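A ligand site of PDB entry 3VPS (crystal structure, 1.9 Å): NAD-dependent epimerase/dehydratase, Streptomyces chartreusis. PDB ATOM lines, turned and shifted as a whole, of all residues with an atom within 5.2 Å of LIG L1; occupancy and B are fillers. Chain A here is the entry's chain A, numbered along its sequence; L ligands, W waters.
The backbone NH of Glu 121 lies within hydrogen-bond range of the side-chain hydroxyl of Thr 119 (3.0 Å).
NZ of Lys 80 is in salt-bridge range of OE2 of Glu 179 (3.4 Å).
The side-chain carboxylate (OE1) of Glu 267 lies within salt-bridge range of the guanidinium group (NH2) of Arg 208 (2.8 Å).
OE1 of Glu 201 lies within salt-bridge range of NE of Arg 264 (3.0 Å).
The side-chain carboxylate (OE2) of Glu 201 lies within salt-bridge range of the guanidinium group (NH1) of Arg 187, 3.3 Å away.
The side-chain amide nitrogen of Gln 206 sits at hydrogen-bond distance from the backbone carbonyl oxygen of Glu 201 (2.8 Å).
O of Phe 171 lies within hydrogen-bond range of N of Cys 120 (2.9 Å).
The backbone carbonyl oxygen of Gln 206 is in hydrogen-bond range of the backbone NH of Val 242 (2.9 Å).
Merely in contact with LIG L1: Ala 183 (3.4 Å), Val 200 (3.5 Å), Val 242 (3.5 Å), Glu 179 (3.6 Å), Asp 182 (3.6 Å), Val 82 (3.7 Å), Phe 171 (3.95 Å) and Phe 271 (3.98 Å).
Hydrophobic or aromatic side chains within 4 Å of LIG L1: Val 82, Tyr 143, Ala 183, Leu 184, Pro 199, Val 242 and Phe 271.
Within 4 Å of LIG L1: Lys 80, Val 82, Thr 119, Cys 120, Glu 121, Tyr 143, Phe 171, Asn 173, Glu 179, Asp 182, Ala 183, Leu 184, Arg 187, Pro 199, Val 200, Glu 201, Gln 206, Arg 208, Val 242, Arg 264, Glu 267 and Phe 271.
The nearest printed residue that does not touch LIG L1 is Leu 188 (4.2 Å).
Water W2 lies within hydrogen-bond range of O17 of LIG L1 (2.7 Å), OE2 of Glu 121 (2.8 Å) and NH2 of Arg 208 (3.3 Å).
Water W1 lies within hydrogen-bond range of O17 of LIG L1 (2.9 Å) and N of Val 82 (2.9 Å).
OG1 of Thr 119 lies within hydrogen-bond range of O3 of LIG L1 (2.5 Å).
N of Leu 184 is in hydrogen-bond range of O13 of LIG L1 (2.5 Å).
An oxygen (O2) of LIG L1 sits at hydrogen-bond distance from the backbone carbonyl oxygen (O) of Lys 80, at 2.6 Å.
The side-chain amino group (NZ) of Lys 80 sits at hydrogen-bond distance from an oxygen (O6) of LIG L1, at 2.8 Å.
OE2 of Glu 267 sits at hydrogen-bond distance from O11 of LIG L1 (2.6 Å).
The backbone NH (N) of Glu 201 sits at hydrogen-bond distance from an oxygen (O7) of LIG L1.
An oxygen (O9) of LIG L1 is in hydrogen-bond range of the side-chain carboxylate of Glu 201, 2.6 Å away.
The side-chain hydroxyl (OH) of Tyr 143 lies within hydrogen-bond range of an oxygen (O3) of LIG L1.
SG of Cys 120 lies within hydrogen-bond range of O5 of LIG L1, 2.7 Å away.
NH1 of Arg 264 is in salt-bridge range of O17 of LIG L1 (2.8 Å).
NH1 of Arg 187 sits at hydrogen-bond distance from O8 of LIG L1, at 2.8 Å.
A nitrogen (N3) of LIG L1 lies within hydrogen-bond range of the backbone carbonyl oxygen of Pro 199 (2.9 Å).
An oxygen (O16) of LIG L1 lies within salt-bridge range of the guanidinium group (NE) of Arg 208.
OE2 of Glu 121 lies within hydrogen-bond range of O5 of LIG L1 (3.1 Å).
ND2 of Asn 173 lies within hydrogen-bond range of O5 of LIG L1, 3.1 Å away.
The side-chain amide nitrogen of Gln 206 lies close to an oxygen (O11) of LIG L1, at 3.4 Å.
The side-chain amino group of Lys 80 is in salt-bridge range of an oxygen (O8) of LG2 L2 (2.8 Å).
O13 of LG2 L2 is in hydrogen-bond range of OH of Tyr 143, at 3.0 Å.
The side-chain carboxylate of Glu 179 is in hydrogen-bond range of a nitrogen (N7) of LG2 L2, 3.3 Å away.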
ATOM      1  N   LYS A  80      18.771   3.373 -30.407  1.00  0.00           N
ATOM      2  CA  LYS A  80      20.025   3.998 -29.929  1.00  0.00           C
ATOM      3  C   LYS A  80      19.932   5.496 -29.594  1.00  0.00           C
ATOM      4  O   LYS A  80      20.973   6.124 -29.318  1.00  0.00           O
ATOM      5  CB  LYS A  80      21.250   3.726 -30.872  1.00  0.00           C
ATOM      6  CG  LYS A  80      21.122   4.282 -32.260  1.00  0.00           C
ATOM      7  CD  LYS A  80      22.443   4.880 -32.791  1.00  0.00           C
ATOM      8  CE  LYS A  80      22.205   5.647 -34.124  1.00  0.00           C
ATOM      9  NZ  LYS A  80      23.529   6.186 -34.710  1.00  0.00           N
ATOM     10  N   SER A  81      18.721   6.056 -29.592  1.00  0.00           N
ATOM     11  CA  SER A  81      18.563   7.523 -29.418  1.00  0.00           C
ATOM     12  C   SER A  81      18.344   7.944 -27.957  1.00  0.00           C
ATOM     13  O   SER A  81      17.312   7.606 -27.330  1.00  0.00           O
ATOM     14  CB  SER A  81      17.411   8.062 -30.267  1.00  0.00           C
ATOM     15  OG  SER A  81      17.049   9.379 -29.820  1.00  0.00           O
ATOM     16  N   VAL A  82      19.303   8.705 -27.432  1.00  0.00           N
ATOM     17  CA  VAL A  82      19.214   9.116 -26.049  1.00  0.00           C
ATOM     18  C   VAL A  82      17.932   9.963 -25.891  1.00  0.00           C
ATOM     19  O   VAL A  82      17.075   9.590 -25.070  1.00  0.00           O
ATOM     20  CB  VAL A  82      20.488   9.848 -25.594  1.00  0.00           C
ATOM     21  CG1 VAL A  82      20.310  10.396 -24.157  1.00  0.00           C
ATOM     22  CG2 VAL A  82      21.704   8.952 -25.714  1.00  0.00           C
ATOM     23  N   PRO A  83      17.785  11.079 -26.671  1.00  0.00           N
ATOM     24  CA  PRO A  83      16.656  12.008 -26.379  1.00  0.00           C
ATOM     25  C   PRO A  83      15.299  11.319 -26.601  1.00  0.00           C
ATOM     26  O   PRO A  83      14.351  11.529 -25.819  1.00  0.00           O
ATOM     27  CB  PRO A  83      16.844  13.177 -27.388  1.00  0.00           C
ATOM     28  CG  PRO A  83      17.829  12.646 -28.447  1.00  0.00           C
ATOM     29  CD  PRO A  83      18.680  11.611 -27.734  1.00  0.00           C
ATOM     30  N   THR A 119      27.610   1.123 -24.701  1.00  0.00           N
ATOM     31  CA  THR A 119      27.820   2.539 -24.967  1.00  0.00           C
ATOM     32  C   THR A 119      28.423   3.195 -23.724  1.00  0.00           C
ATOM     33  O   THR A 119      28.137   2.782 -22.597  1.00  0.00           O
ATOM     34  CB  THR A 119      26.470   3.231 -25.297  1.00  0.00           C
ATOM     35  OG1 THR A 119      26.654   4.649 -25.293  1.00  0.00           O
ATOM     36  CG2 THR A 119      25.426   2.858 -24.256  1.00  0.00           C
ATOM     37  N   CYS A 120      29.168   4.268 -23.954  1.00  0.00           N
ATOM     38  CA  CYS A 120      29.652   5.121 -22.837  1.00  0.00           C
ATOM     39  C   CYS A 120      28.488   5.694 -22.031  1.00  0.00           C
ATOM     40  O   CYS A 120      28.698   6.097 -20.921  1.00  0.00           O
ATOM     41  CB  CYS A 120      30.565   6.216 -23.376  1.00  0.00           C
ATOM     42  SG  CYS A 120      29.793   7.350 -24.537  1.00  0.00           S
ATOM     43  N   GLU A 121      27.263   5.704 -22.579  1.00  0.00           N
ATOM     44  CA  GLU A 121      26.151   6.345 -21.858  1.00  0.00           C
ATOM     45  C   GLU A 121      25.884   5.623 -20.540  1.00  0.00           C
ATOM     46  O   GLU A 121      25.259   6.179 -19.635  1.00  0.00           O
ATOM     47  CB  GLU A 121      24.801   6.450 -22.677  1.00  0.00           C
ATOM     48  CG  GLU A 121      24.950   7.242 -23.956  1.00  0.00           C
ATOM     49  CD  GLU A 121      24.822   8.686 -23.812  1.00  0.00           C
ATOM     50  OE1 GLU A 121      24.109   9.176 -22.885  1.00  0.00           O
ATOM     51  OE2 GLU A 121      25.426   9.383 -24.682  1.00  0.00           O
ATOM     52  N   TYR A 143      17.275   5.112 -22.559  1.00  0.00           N
ATOM     53  CA  TYR A 143      18.151   4.388 -23.460  1.00  0.00           C
ATOM     54  C   TYR A 143      19.377   3.831 -22.700  1.00  0.00           C
ATOM     55  O   TYR A 143      19.730   2.681 -22.845  1.00  0.00           O
ATOM     56  CB  TYR A 143      18.590   5.244 -24.708  1.00  0.00           C
ATOM     57  CG  TYR A 143      19.882   4.742 -25.383  1.00  0.00           C
ATOM     58  CD1 TYR A 143      19.901   3.591 -26.195  1.00  0.00           C
ATOM     59  CD2 TYR A 143      21.073   5.416 -25.183  1.00  0.00           C
ATOM     60  CE1 TYR A 143      21.134   3.113 -26.808  1.00  0.00           C
ATOM     61  CE2 TYR A 143      22.286   4.968 -25.734  1.00  0.00           C
ATOM     62  CZ  TYR A 143      22.303   3.808 -26.567  1.00  0.00           C
ATOM     63  OH  TYR A 143      23.517   3.415 -27.075  1.00  0.00           O
ATOM     64  N   PHE A 171      31.015   1.610 -26.911  1.00  0.00           N
ATOM     65  CA  PHE A 171      31.367   2.567 -27.924  1.00  0.00           C
ATOM     66  C   PHE A 171      31.214   3.988 -27.380  1.00  0.00           C
ATOM     67  O   PHE A 171      30.228   4.276 -26.702  1.00  0.00           O
ATOM     68  CB  PHE A 171      30.440   2.453 -29.137  1.00  0.00           C
ATOM     69  CG  PHE A 171      30.577   1.211 -29.874  1.00  0.00           C
ATOM     70  CD1 PHE A 171      31.681   0.986 -30.718  1.00  0.00           C
ATOM     71  CD2 PHE A 171      29.589   0.219 -29.772  1.00  0.00           C
ATOM     72  CE1 PHE A 171      31.792  -0.173 -31.458  1.00  0.00           C
ATOM     73  CE2 PHE A 171      29.708  -0.961 -30.487  1.00  0.00           C
ATOM     74  CZ  PHE A 171      30.776  -1.178 -31.329  1.00  0.00           C
ATOM     75  N   PHE A 172      32.163   4.858 -27.690  1.00  0.00           N
ATOM     76  CA  PHE A 172      31.977   6.277 -27.461  1.00  0.00           C
ATOM     77  C   PHE A 172      31.418   6.823 -28.773  1.00  0.00           C
ATOM     78  O   PHE A 172      30.877   6.022 -29.553  1.00  0.00           O
ATOM     79  CB  PHE A 172      33.252   6.974 -26.925  1.00  0.00           C
ATOM     80  CG  PHE A 172      33.562   6.616 -25.494  1.00  0.00           C
ATOM     81  CD1 PHE A 172      33.506   7.589 -24.510  1.00  0.00           C
ATOM     82  CD2 PHE A 172      33.858   5.260 -25.110  1.00  0.00           C
ATOM     83  CE1 PHE A 172      33.758   7.294 -23.145  1.00  0.00           C
ATOM     84  CE2 PHE A 172      34.112   4.937 -23.781  1.00  0.00           C
ATOM     85  CZ  PHE A 172      34.084   5.978 -22.782  1.00  0.00           C
ATOM     86  N   ASN A 173      31.374   8.109 -29.015  1.00  0.00           N
ATOM     87  CA  ASN A 173      30.668   8.605 -30.180  1.00  0.00           C
ATOM     88  C   ASN A 173      31.340   8.188 -31.486  1.00  0.00           C
ATOM     89  O   ASN A 173      32.457   8.640 -31.761  1.00  0.00           O
ATOM     90  CB  ASN A 173      30.553  10.139 -30.139  1.00  0.00           C
ATOM     91  CG  ASN A 173      29.497  10.604 -29.153  1.00  0.00           C
ATOM     92  OD1 ASN A 173      28.486  11.235 -29.544  1.00  0.00           O
ATOM     93  ND2 ASN A 173      29.690  10.294 -27.921  1.00  0.00           N
ATOM     94  N   GLU A 179      26.038   7.261 -41.405  1.00  0.00           N
ATOM     95  CA  GLU A 179      25.359   7.404 -40.171  1.00  0.00           C
ATOM     96  C   GLU A 179      24.132   8.369 -40.391  1.00  0.00           C
ATOM     97  O   GLU A 179      24.281   9.445 -40.982  1.00  0.00           O
ATOM     98  CB  GLU A 179      26.316   7.954 -39.079  1.00  0.00           C
ATOM     99  CG  GLU A 179      25.624   8.035 -37.705  1.00  0.00           C
ATOM    100  CD  GLU A 179      26.511   8.526 -36.565  1.00  0.00           C
ATOM    101  OE1 GLU A 179      27.274   9.525 -36.766  1.00  0.00           O
ATOM    102  OE2 GLU A 179      26.423   7.898 -35.462  1.00  0.00           O
ATOM    103  N   ASP A 182      20.518  11.843 -37.107  1.00  0.00           N
ATOM    104  CA  ASP A 182      20.006  12.270 -35.785  1.00  0.00           C
ATOM    105  C   ASP A 182      21.191  12.516 -34.810  1.00  0.00           C
ATOM    106  O   ASP A 182      21.077  13.326 -33.864  1.00  0.00           O
ATOM    107  CB  ASP A 182      18.938  11.321 -35.212  1.00  0.00           C
ATOM    108  CG  ASP A 182      19.476   9.898 -34.935  1.00  0.00           C
ATOM    109  OD1 ASP A 182      20.414   9.458 -35.637  1.00  0.00           O
ATOM    110  OD2 ASP A 182      18.948   9.203 -34.031  1.00  0.00           O
ATOM    111  N   ALA A 183      22.346  11.955 -35.155  1.00  0.00           N
ATOM    112  CA  ALA A 183      23.600  12.174 -34.445  1.00  0.00           C
ATOM    113  C   ALA A 183      24.292  13.466 -34.874  1.00  0.00           C
ATOM    114  O   ALA A 183      24.186  13.826 -36.032  1.00  0.00           O
ATOM    115  CB  ALA A 183      24.612  10.988 -34.737  1.00  0.00           C
ATOM    116  N   LEU A 184      25.117  14.019 -34.009  1.00  0.00           N
ATOM    117  CA  LEU A 184      25.723  15.344 -34.196  1.00  0.00           C
ATOM    118  C   LEU A 184      26.388  15.571 -35.570  1.00  0.00           C
ATOM    119  O   LEU A 184      25.994  16.463 -36.333  1.00  0.00           O
ATOM    120  CB  LEU A 184      26.766  15.613 -33.104  1.00  0.00           C
ATOM    121  CG  LEU A 184      27.460  16.997 -33.196  1.00  0.00           C
ATOM    122  CD1 LEU A 184      26.489  18.122 -32.842  1.00  0.00           C
ATOM    123  CD2 LEU A 184      28.734  17.050 -32.318  1.00  0.00           C
ATOM    124  N   VAL A 185      27.426  14.809 -35.873  1.00  0.00           N
ATOM    125  CA  VAL A 185      28.170  15.114 -37.076  1.00  0.00           C
ATOM    126  C   VAL A 185      27.261  15.069 -38.337  1.00  0.00           C
ATOM    127  O   VAL A 185      27.212  16.046 -39.077  1.00  0.00           O
ATOM    128  CB  VAL A 185      29.433  14.287 -37.222  1.00  0.00           C
ATOM    129  CG1 VAL A 185      30.149  14.622 -38.542  1.00  0.00           C
ATOM    130  CG2 VAL A 185      30.339  14.528 -36.049  1.00  0.00           C
ATOM    131  N   ARG A 187      24.063  15.259 -38.442  1.00  0.00           N
ATOM    132  CA  ARG A 187      22.995  16.270 -38.321  1.00  0.00           C
ATOM    133  C   ARG A 187      23.528  17.588 -38.793  1.00  0.00           C
ATOM    134  O   ARG A 187      22.876  18.230 -39.609  1.00  0.00           O
ATOM    135  CB  ARG A 187      22.415  16.359 -36.914  1.00  0.00           C
ATOM    136  CG  ARG A 187      21.096  17.134 -36.903  1.00  0.00           C
ATOM    137  CD  ARG A 187      20.142  16.726 -35.796  1.00  0.00           C
ATOM    138  NE  ARG A 187      19.070  17.718 -35.686  1.00  0.00           N
ATOM    139  CZ  ARG A 187      18.834  18.433 -34.617  1.00  0.00           C
ATOM    140  NH1 ARG A 187      19.568  18.181 -33.625  1.00  0.00           N
ATOM    141  NH2 ARG A 187      17.882  19.353 -34.475  1.00  0.00           N
ATOM    142  N   LEU A 188      24.724  17.952 -38.337  1.00  0.00           N
ATOM    143  CA  LEU A 188      25.351  19.209 -38.726  1.00  0.00           C
ATOM    144  C   LEU A 188      25.566  19.265 -40.229  1.00  0.00           C
ATOM    145  O   LEU A 188      25.264  20.267 -40.866  1.00  0.00           O
ATOM    146  CB  LEU A 188      26.677  19.379 -38.011  1.00  0.00           C
ATOM    147  CG  LEU A 188      26.578  19.597 -36.491  1.00  0.00           C
ATOM    148  CD1 LEU A 188      27.911  20.000 -35.928  1.00  0.00           C
ATOM    149  CD2 LEU A 188      25.503  20.612 -36.144  1.00  0.00           C
ATOM    150  N   PRO A 199      22.810  23.545 -35.924  1.00  0.00           N
ATOM    151  CA  PRO A 199      22.046  23.505 -34.667  1.00  0.00           C
ATOM    152  C   PRO A 199      22.898  23.121 -33.455  1.00  0.00           C
ATOM    153  O   PRO A 199      23.616  22.115 -33.522  1.00  0.00           O
ATOM    154  CB  PRO A 199      20.971  22.435 -34.914  1.00  0.00           C
ATOM    155  CG  PRO A 199      21.445  21.663 -36.094  1.00  0.00           C
ATOM    156  CD  PRO A 199      22.458  22.456 -36.852  1.00  0.00           C
ATOM    157  N   VAL A 200      22.838  23.932 -32.404  1.00  0.00           N
ATOM    158  CA  VAL A 200      23.526  23.611 -31.148  1.00  0.00           C
ATOM    159  C   VAL A 200      22.501  23.513 -30.016  1.00  0.00           C
ATOM    160  O   VAL A 200      21.773  24.472 -29.753  1.00  0.00           O
ATOM    161  CB  VAL A 200      24.593  24.659 -30.781  1.00  0.00           C
ATOM    162  CG1 VAL A 200      25.239  24.333 -29.465  1.00  0.00           C
ATOM    163  CG2 VAL A 200      25.643  24.711 -31.853  1.00  0.00           C
ATOM    164  N   GLU A 201      22.444  22.343 -29.386  1.00  0.00           N
ATOM    165  CA  GLU A 201      21.539  22.108 -28.285  1.00  0.00           C
ATOM    166  C   GLU A 201      22.245  22.571 -27.022  1.00  0.00           C
ATOM    167  O   GLU A 201      23.311  22.051 -26.707  1.00  0.00           O
ATOM    168  CB  GLU A 201      21.182  20.613 -28.231  1.00  0.00           C
ATOM    169  CG  GLU A 201      20.321  20.188 -29.409  1.00  0.00           C
ATOM    170  CD  GLU A 201      20.026  18.709 -29.436  1.00  0.00           C
ATOM    171  OE1 GLU A 201      20.516  17.955 -28.571  1.00  0.00           O
ATOM    172  OE2 GLU A 201      19.303  18.277 -30.346  1.00  0.00           O
ATOM    173  N   GLN A 206      29.329  21.151 -23.949  1.00  0.00           N
ATOM    174  CA  GLN A 206      29.311  19.713 -23.665  1.00  0.00           C
ATOM    175  C   GLN A 206      30.293  19.008 -24.606  1.00  0.00           C
ATOM    176  O   GLN A 206      30.465  19.462 -25.761  1.00  0.00           O
ATOM    177  CB  GLN A 206      27.911  19.119 -23.762  1.00  0.00           C
ATOM    178  CG  GLN A 206      27.282  19.084 -25.184  1.00  0.00           C
ATOM    179  CD  GLN A 206      26.463  20.358 -25.477  1.00  0.00           C
ATOM    180  OE1 GLN A 206      26.779  21.424 -24.987  1.00  0.00           O
ATOM    181  NE2 GLN A 206      25.386  20.227 -26.255  1.00  0.00           N
ATOM    182  N   ARG A 208      32.333  15.333 -26.183  1.00  0.00           N
ATOM    183  CA  ARG A 208      32.200  13.943 -26.550  1.00  0.00           C
ATOM    184  C   ARG A 208      33.541  13.455 -27.056  1.00  0.00           C
ATOM    185  O   ARG A 208      34.421  14.245 -27.472  1.00  0.00           O
ATOM    186  CB  ARG A 208      31.109  13.754 -27.627  1.00  0.00           C
ATOM    187  CG  ARG A 208      29.707  14.069 -27.150  1.00  0.00           C
ATOM    188  CD  ARG A 208      29.237  13.125 -26.041  1.00  0.00           C
ATOM    189  NE  ARG A 208      27.823  13.338 -25.648  1.00  0.00           N
ATOM    190  CZ  ARG A 208      27.383  14.165 -24.699  1.00  0.00           C
ATOM    191  NH1 ARG A 208      28.222  14.970 -24.058  1.00  0.00           N
ATOM    192  NH2 ARG A 208      26.067  14.223 -24.437  1.00  0.00           N
ATOM    193  N   VAL A 242      30.983  20.261 -28.495  1.00  0.00           N
ATOM    194  CA  VAL A 242      30.098  20.543 -29.635  1.00  0.00           C
ATOM    195  C   VAL A 242      30.547  21.830 -30.410  1.00  0.00           C
ATOM    196  O   VAL A 242      30.621  21.817 -31.658  1.00  0.00           O
ATOM    197  CB  VAL A 242      28.595  20.577 -29.206  1.00  0.00           C
ATOM    198  CG1 VAL A 242      27.691  21.027 -30.376  1.00  0.00           C
ATOM    199  CG2 VAL A 242      28.176  19.167 -28.682  1.00  0.00           C
ATOM    200  N   ARG A 264      19.550  19.415 -23.913  1.00  0.00           N
ATOM    201  CA  ARG A 264      18.960  18.162 -23.607  1.00  0.00           C
ATOM    202  C   ARG A 264      18.662  18.057 -22.125  1.00  0.00           C
ATOM    203  O   ARG A 264      19.341  18.629 -21.334  1.00  0.00           O
ATOM    204  CB  ARG A 264      19.892  17.035 -24.032  1.00  0.00           C
ATOM    205  CG  ARG A 264      20.042  16.911 -25.500  1.00  0.00           C
ATOM    206  CD  ARG A 264      20.023  15.483 -25.856  1.00  0.00           C
ATOM    207  NE  ARG A 264      20.129  15.267 -27.298  1.00  0.00           N
ATOM    208  CZ  ARG A 264      21.063  14.504 -27.841  1.00  0.00           C
ATOM    209  NH1 ARG A 264      21.951  13.895 -27.090  1.00  0.00           N
ATOM    210  NH2 ARG A 264      21.108  14.341 -29.155  1.00  0.00           N
ATOM    211  N   GLU A 267      21.615  16.288 -19.373  1.00  0.00           N
ATOM    212  CA  GLU A 267      22.727  16.338 -20.329  1.00  0.00           C
ATOM    213  C   GLU A 267      24.000  15.904 -19.636  1.00  0.00           C
ATOM    214  O   GLU A 267      24.166  16.112 -18.436  1.00  0.00           O
ATOM    215  CB  GLU A 267      22.905  17.775 -20.886  1.00  0.00           C
ATOM    216  CG  GLU A 267      24.021  17.932 -21.953  1.00  0.00           C
ATOM    217  CD  GLU A 267      23.911  16.918 -23.150  1.00  0.00           C
ATOM    218  OE1 GLU A 267      24.135  15.697 -22.974  1.00  0.00           O
ATOM    219  OE2 GLU A 267      23.649  17.365 -24.299  1.00  0.00           O
ATOM    220  N   PHE A 271      31.977  13.048 -22.023  1.00  0.00           N
ATOM    221  CA  PHE A 271      32.425  11.651 -22.100  1.00  0.00           C
ATOM    222  C   PHE A 271      33.860  11.673 -22.626  1.00  0.00           C
ATOM    223  O   PHE A 271      34.161  12.430 -23.556  1.00  0.00           O
ATOM    224  CB  PHE A 271      31.621  10.840 -23.083  1.00  0.00           C
ATOM    225  CG  PHE A 271      30.259  10.515 -22.645  1.00  0.00           C
ATOM    226  CD1 PHE A 271      30.010   9.614 -21.585  1.00  0.00           C
ATOM    227  CD2 PHE A 271      29.179  11.081 -23.323  1.00  0.00           C
ATOM    228  CE1 PHE A 271      28.670   9.291 -21.219  1.00  0.00           C
ATOM    229  CE2 PHE A 271      27.844  10.776 -22.946  1.00  0.00           C
ATOM    230  CZ  PHE A 271      27.603   9.845 -21.883  1.00  0.00           C
HETATM  231  C1  LIG L   1      25.517   8.928 -29.383  1.00  0.00           C
HETATM  232  C2  LIG L   1      24.703   7.744 -29.939  1.00  0.00           C
HETATM  233  C3  LIG L   1      24.252   6.779 -28.842  1.00  0.00           C
HETATM  234  C4  LIG L   1      25.472   6.381 -28.014  1.00  0.00           C
HETATM  235  C5  LIG L   1      26.335   7.591 -27.607  1.00  0.00           C
HETATM  236  C6  LIG L   1      27.618   7.241 -26.870  1.00  0.00           C
HETATM  237  C7  LIG L   1      23.364   8.425 -31.872  1.00  0.00           C
HETATM  238  C8  LIG L   1      22.096   9.096 -32.281  1.00  0.00           C
HETATM  239  N1  LIG L   1      23.500   8.303 -30.532  1.00  0.00           N
HETATM  240  O1  LIG L   1      24.710   9.623 -28.378  1.00  0.00           O
HETATM  241  O2  LIG L   1      23.517   5.643 -29.401  1.00  0.00           O
HETATM  242  O3  LIG L   1      25.035   5.677 -26.853  1.00  0.00           O
HETATM  243  O4  LIG L   1      26.686   8.456 -28.720  1.00  0.00           O
HETATM  244  O5  LIG L   1      27.921   8.489 -26.198  1.00  0.00           O
HETATM  245  O6  LIG L   1      24.233   8.010 -32.661  1.00  0.00           O
HETATM  246  N2  LIG L   1      23.751  17.951 -30.641  1.00  0.00           N
HETATM  247  C9  LIG L   1      23.743  19.291 -31.144  1.00  0.00           C
HETATM  248  N3  LIG L   1      23.216  19.522 -32.368  1.00  0.00           N
HETATM  249  C10 LIG L   1      22.752  18.494 -33.099  1.00  0.00           C
HETATM  250  C11 LIG L   1      22.783  17.165 -32.647  1.00  0.00           C
HETATM  251  C12 LIG L   1      23.311  16.911 -31.394  1.00  0.00           C
HETATM  252  O7  LIG L   1      24.210  20.260 -30.469  1.00  0.00           O
HETATM  253  O8  LIG L   1      22.290  18.705 -34.223  1.00  0.00           O
HETATM  254  C13 LIG L   1      24.375  17.667 -29.314  1.00  0.00           C
HETATM  255  C14 LIG L   1      23.638  16.799 -28.315  1.00  0.00           C
HETATM  256  O9  LIG L   1      22.867  17.601 -27.428  1.00  0.00           O
HETATM  257  C15 LIG L   1      24.755  16.078 -27.545  1.00  0.00           C
HETATM  258  C16 LIG L   1      25.911  16.043 -28.523  1.00  0.00           C
HETATM  259  O10 LIG L   1      25.593  16.981 -29.579  1.00  0.00           O
HETATM  260  O11 LIG L   1      25.135  16.850 -26.398  1.00  0.00           O
HETATM  261  C17 LIG L   1      26.054  14.660 -29.158  1.00  0.00           C
HETATM  262  O12 LIG L   1      24.749  14.184 -29.461  1.00  0.00           O
HETATM  263  P1  LIG L   1      24.477  12.912 -30.431  1.00  0.00           P
HETATM  264  O13 LIG L   1      25.296  13.154 -31.663  1.00  0.00           O
HETATM  265  O14 LIG L   1      23.011  12.710 -30.566  1.00  0.00           O
HETATM  266  O15 LIG L   1      25.051  11.630 -29.663  1.00  0.00           O
HETATM  267  P2  LIG L   1      24.817  11.179 -28.119  1.00  0.00           P
HETATM  268  O16 LIG L   1      26.094  11.576 -27.430  1.00  0.00           O
HETATM  269  O17 LIG L   1      23.481  11.600 -27.552  1.00  0.00           O
HETATM  270  P1  LG2 L   2      22.036   2.096 -36.441  1.00  0.00           P
HETATM  271  O1  LG2 L   2      20.690   2.685 -36.077  1.00  0.00           O
HETATM  272  O2  LG2 L   2      22.559   2.758 -37.627  1.00  0.00           O
HETATM  273  O3  LG2 L   2      22.006   0.504 -36.569  1.00  0.00           O
HETATM  274  C1  LG2 L   2      21.260  -0.345 -35.732  1.00  0.00           C
HETATM  275  C2  LG2 L   2      20.442  -1.247 -36.665  1.00  0.00           C
HETATM  276  O4  LG2 L   2      19.696  -2.142 -35.851  1.00  0.00           O
HETATM  277  C3  LG2 L   2      19.469  -0.549 -37.582  1.00  0.00           C
HETATM  278  O5  LG2 L   2      19.679  -0.772 -38.987  1.00  0.00           O
HETATM  279  C4  LG2 L   2      18.066  -1.006 -37.104  1.00  0.00           C
HETATM  280  O6  LG2 L   2      17.101  -1.158 -38.122  1.00  0.00           O
HETATM  281  C5  LG2 L   2      18.391  -2.321 -36.473  1.00  0.00           C
HETATM  282  N1  LG2 L   2      17.669  -2.731 -35.290  1.00  0.00           N
HETATM  283  C6  LG2 L   2      17.474  -2.036 -34.121  1.00  0.00           C
HETATM  284  N2  LG2 L   2      16.841  -2.864 -33.246  1.00  0.00           N
HETATM  285  C7  LG2 L   2      16.709  -4.087 -33.851  1.00  0.00           C
HETATM  286  C8  LG2 L   2      16.142  -5.312 -33.426  1.00  0.00           C
HETATM  287  N3  LG2 L   2      15.818  -5.537 -32.133  1.00  0.00           N
HETATM  288  N4  LG2 L   2      16.129  -6.352 -34.329  1.00  0.00           N
HETATM  289  C9  LG2 L   2      16.633  -6.219 -35.615  1.00  0.00           C
HETATM  290  N5  LG2 L   2      17.163  -5.017 -36.026  1.00  0.00           N
HETATM  291  C10 LG2 L   2      17.212  -3.999 -35.130  1.00  0.00           C
HETATM  292  O7  LG2 L   2      22.933   2.379 -35.138  1.00  0.00           O
HETATM  293  P2  LG2 L   2      24.518   2.375 -35.081  1.00  0.00           P
HETATM  294  O8  LG2 L   2      24.953   3.808 -34.957  1.00  0.00           O
HETATM  295  O9  LG2 L   2      25.009   1.548 -36.162  1.00  0.00           O
HETATM  296  O10 LG2 L   2      24.699   1.664 -33.697  1.00  0.00           O
HETATM  297  C11 LG2 L   2      25.006   0.246 -33.597  1.00  0.00           C
HETATM  298  C12 LG2 L   2      25.253  -0.166 -32.141  1.00  0.00           C
HETATM  299  O11 LG2 L   2      26.258   0.665 -31.558  1.00  0.00           O
HETATM  300  C13 LG2 L   2      24.079  -0.084 -31.145  1.00  0.00           C
HETATM  301  O12 LG2 L   2      24.272  -1.181 -30.183  1.00  0.00           O
HETATM  302  C14 LG2 L   2      24.291   1.277 -30.526  1.00  0.00           C
HETATM  303  O13 LG2 L   2      23.652   1.408 -29.309  1.00  0.00           O
HETATM  304  C15 LG2 L   2      25.807   1.261 -30.345  1.00  0.00           C
HETATM  305  N6  LG2 L   2      26.465   2.572 -30.246  1.00  0.00           N
HETATM  306  C16 LG2 L   2      26.608   3.362 -31.365  1.00  0.00           C
HETATM  307  C17 LG2 L   2      27.240   4.592 -31.231  1.00  0.00           C
HETATM  308  C18 LG2 L   2      27.311   5.585 -32.328  1.00  0.00           C
HETATM  309  O14 LG2 L   2      27.811   6.872 -32.277  1.00  0.00           O
HETATM  310  N7  LG2 L   2      26.803   5.297 -33.430  1.00  0.00           N
HETATM  311  C19 LG2 L   2      27.765   4.966 -30.008  1.00  0.00           C
HETATM  312  C20 LG2 L   2      27.611   4.197 -28.883  1.00  0.00           C
HETATM  313  C21 LG2 L   2      26.908   2.993 -28.991  1.00  0.00           C
HETATM  314  O   HOH W   1      21.538   9.885 -28.906  1.00  0.00           O
HETATM  315  O   HOH W   2      23.899  11.770 -24.841  1.00  0.00           O
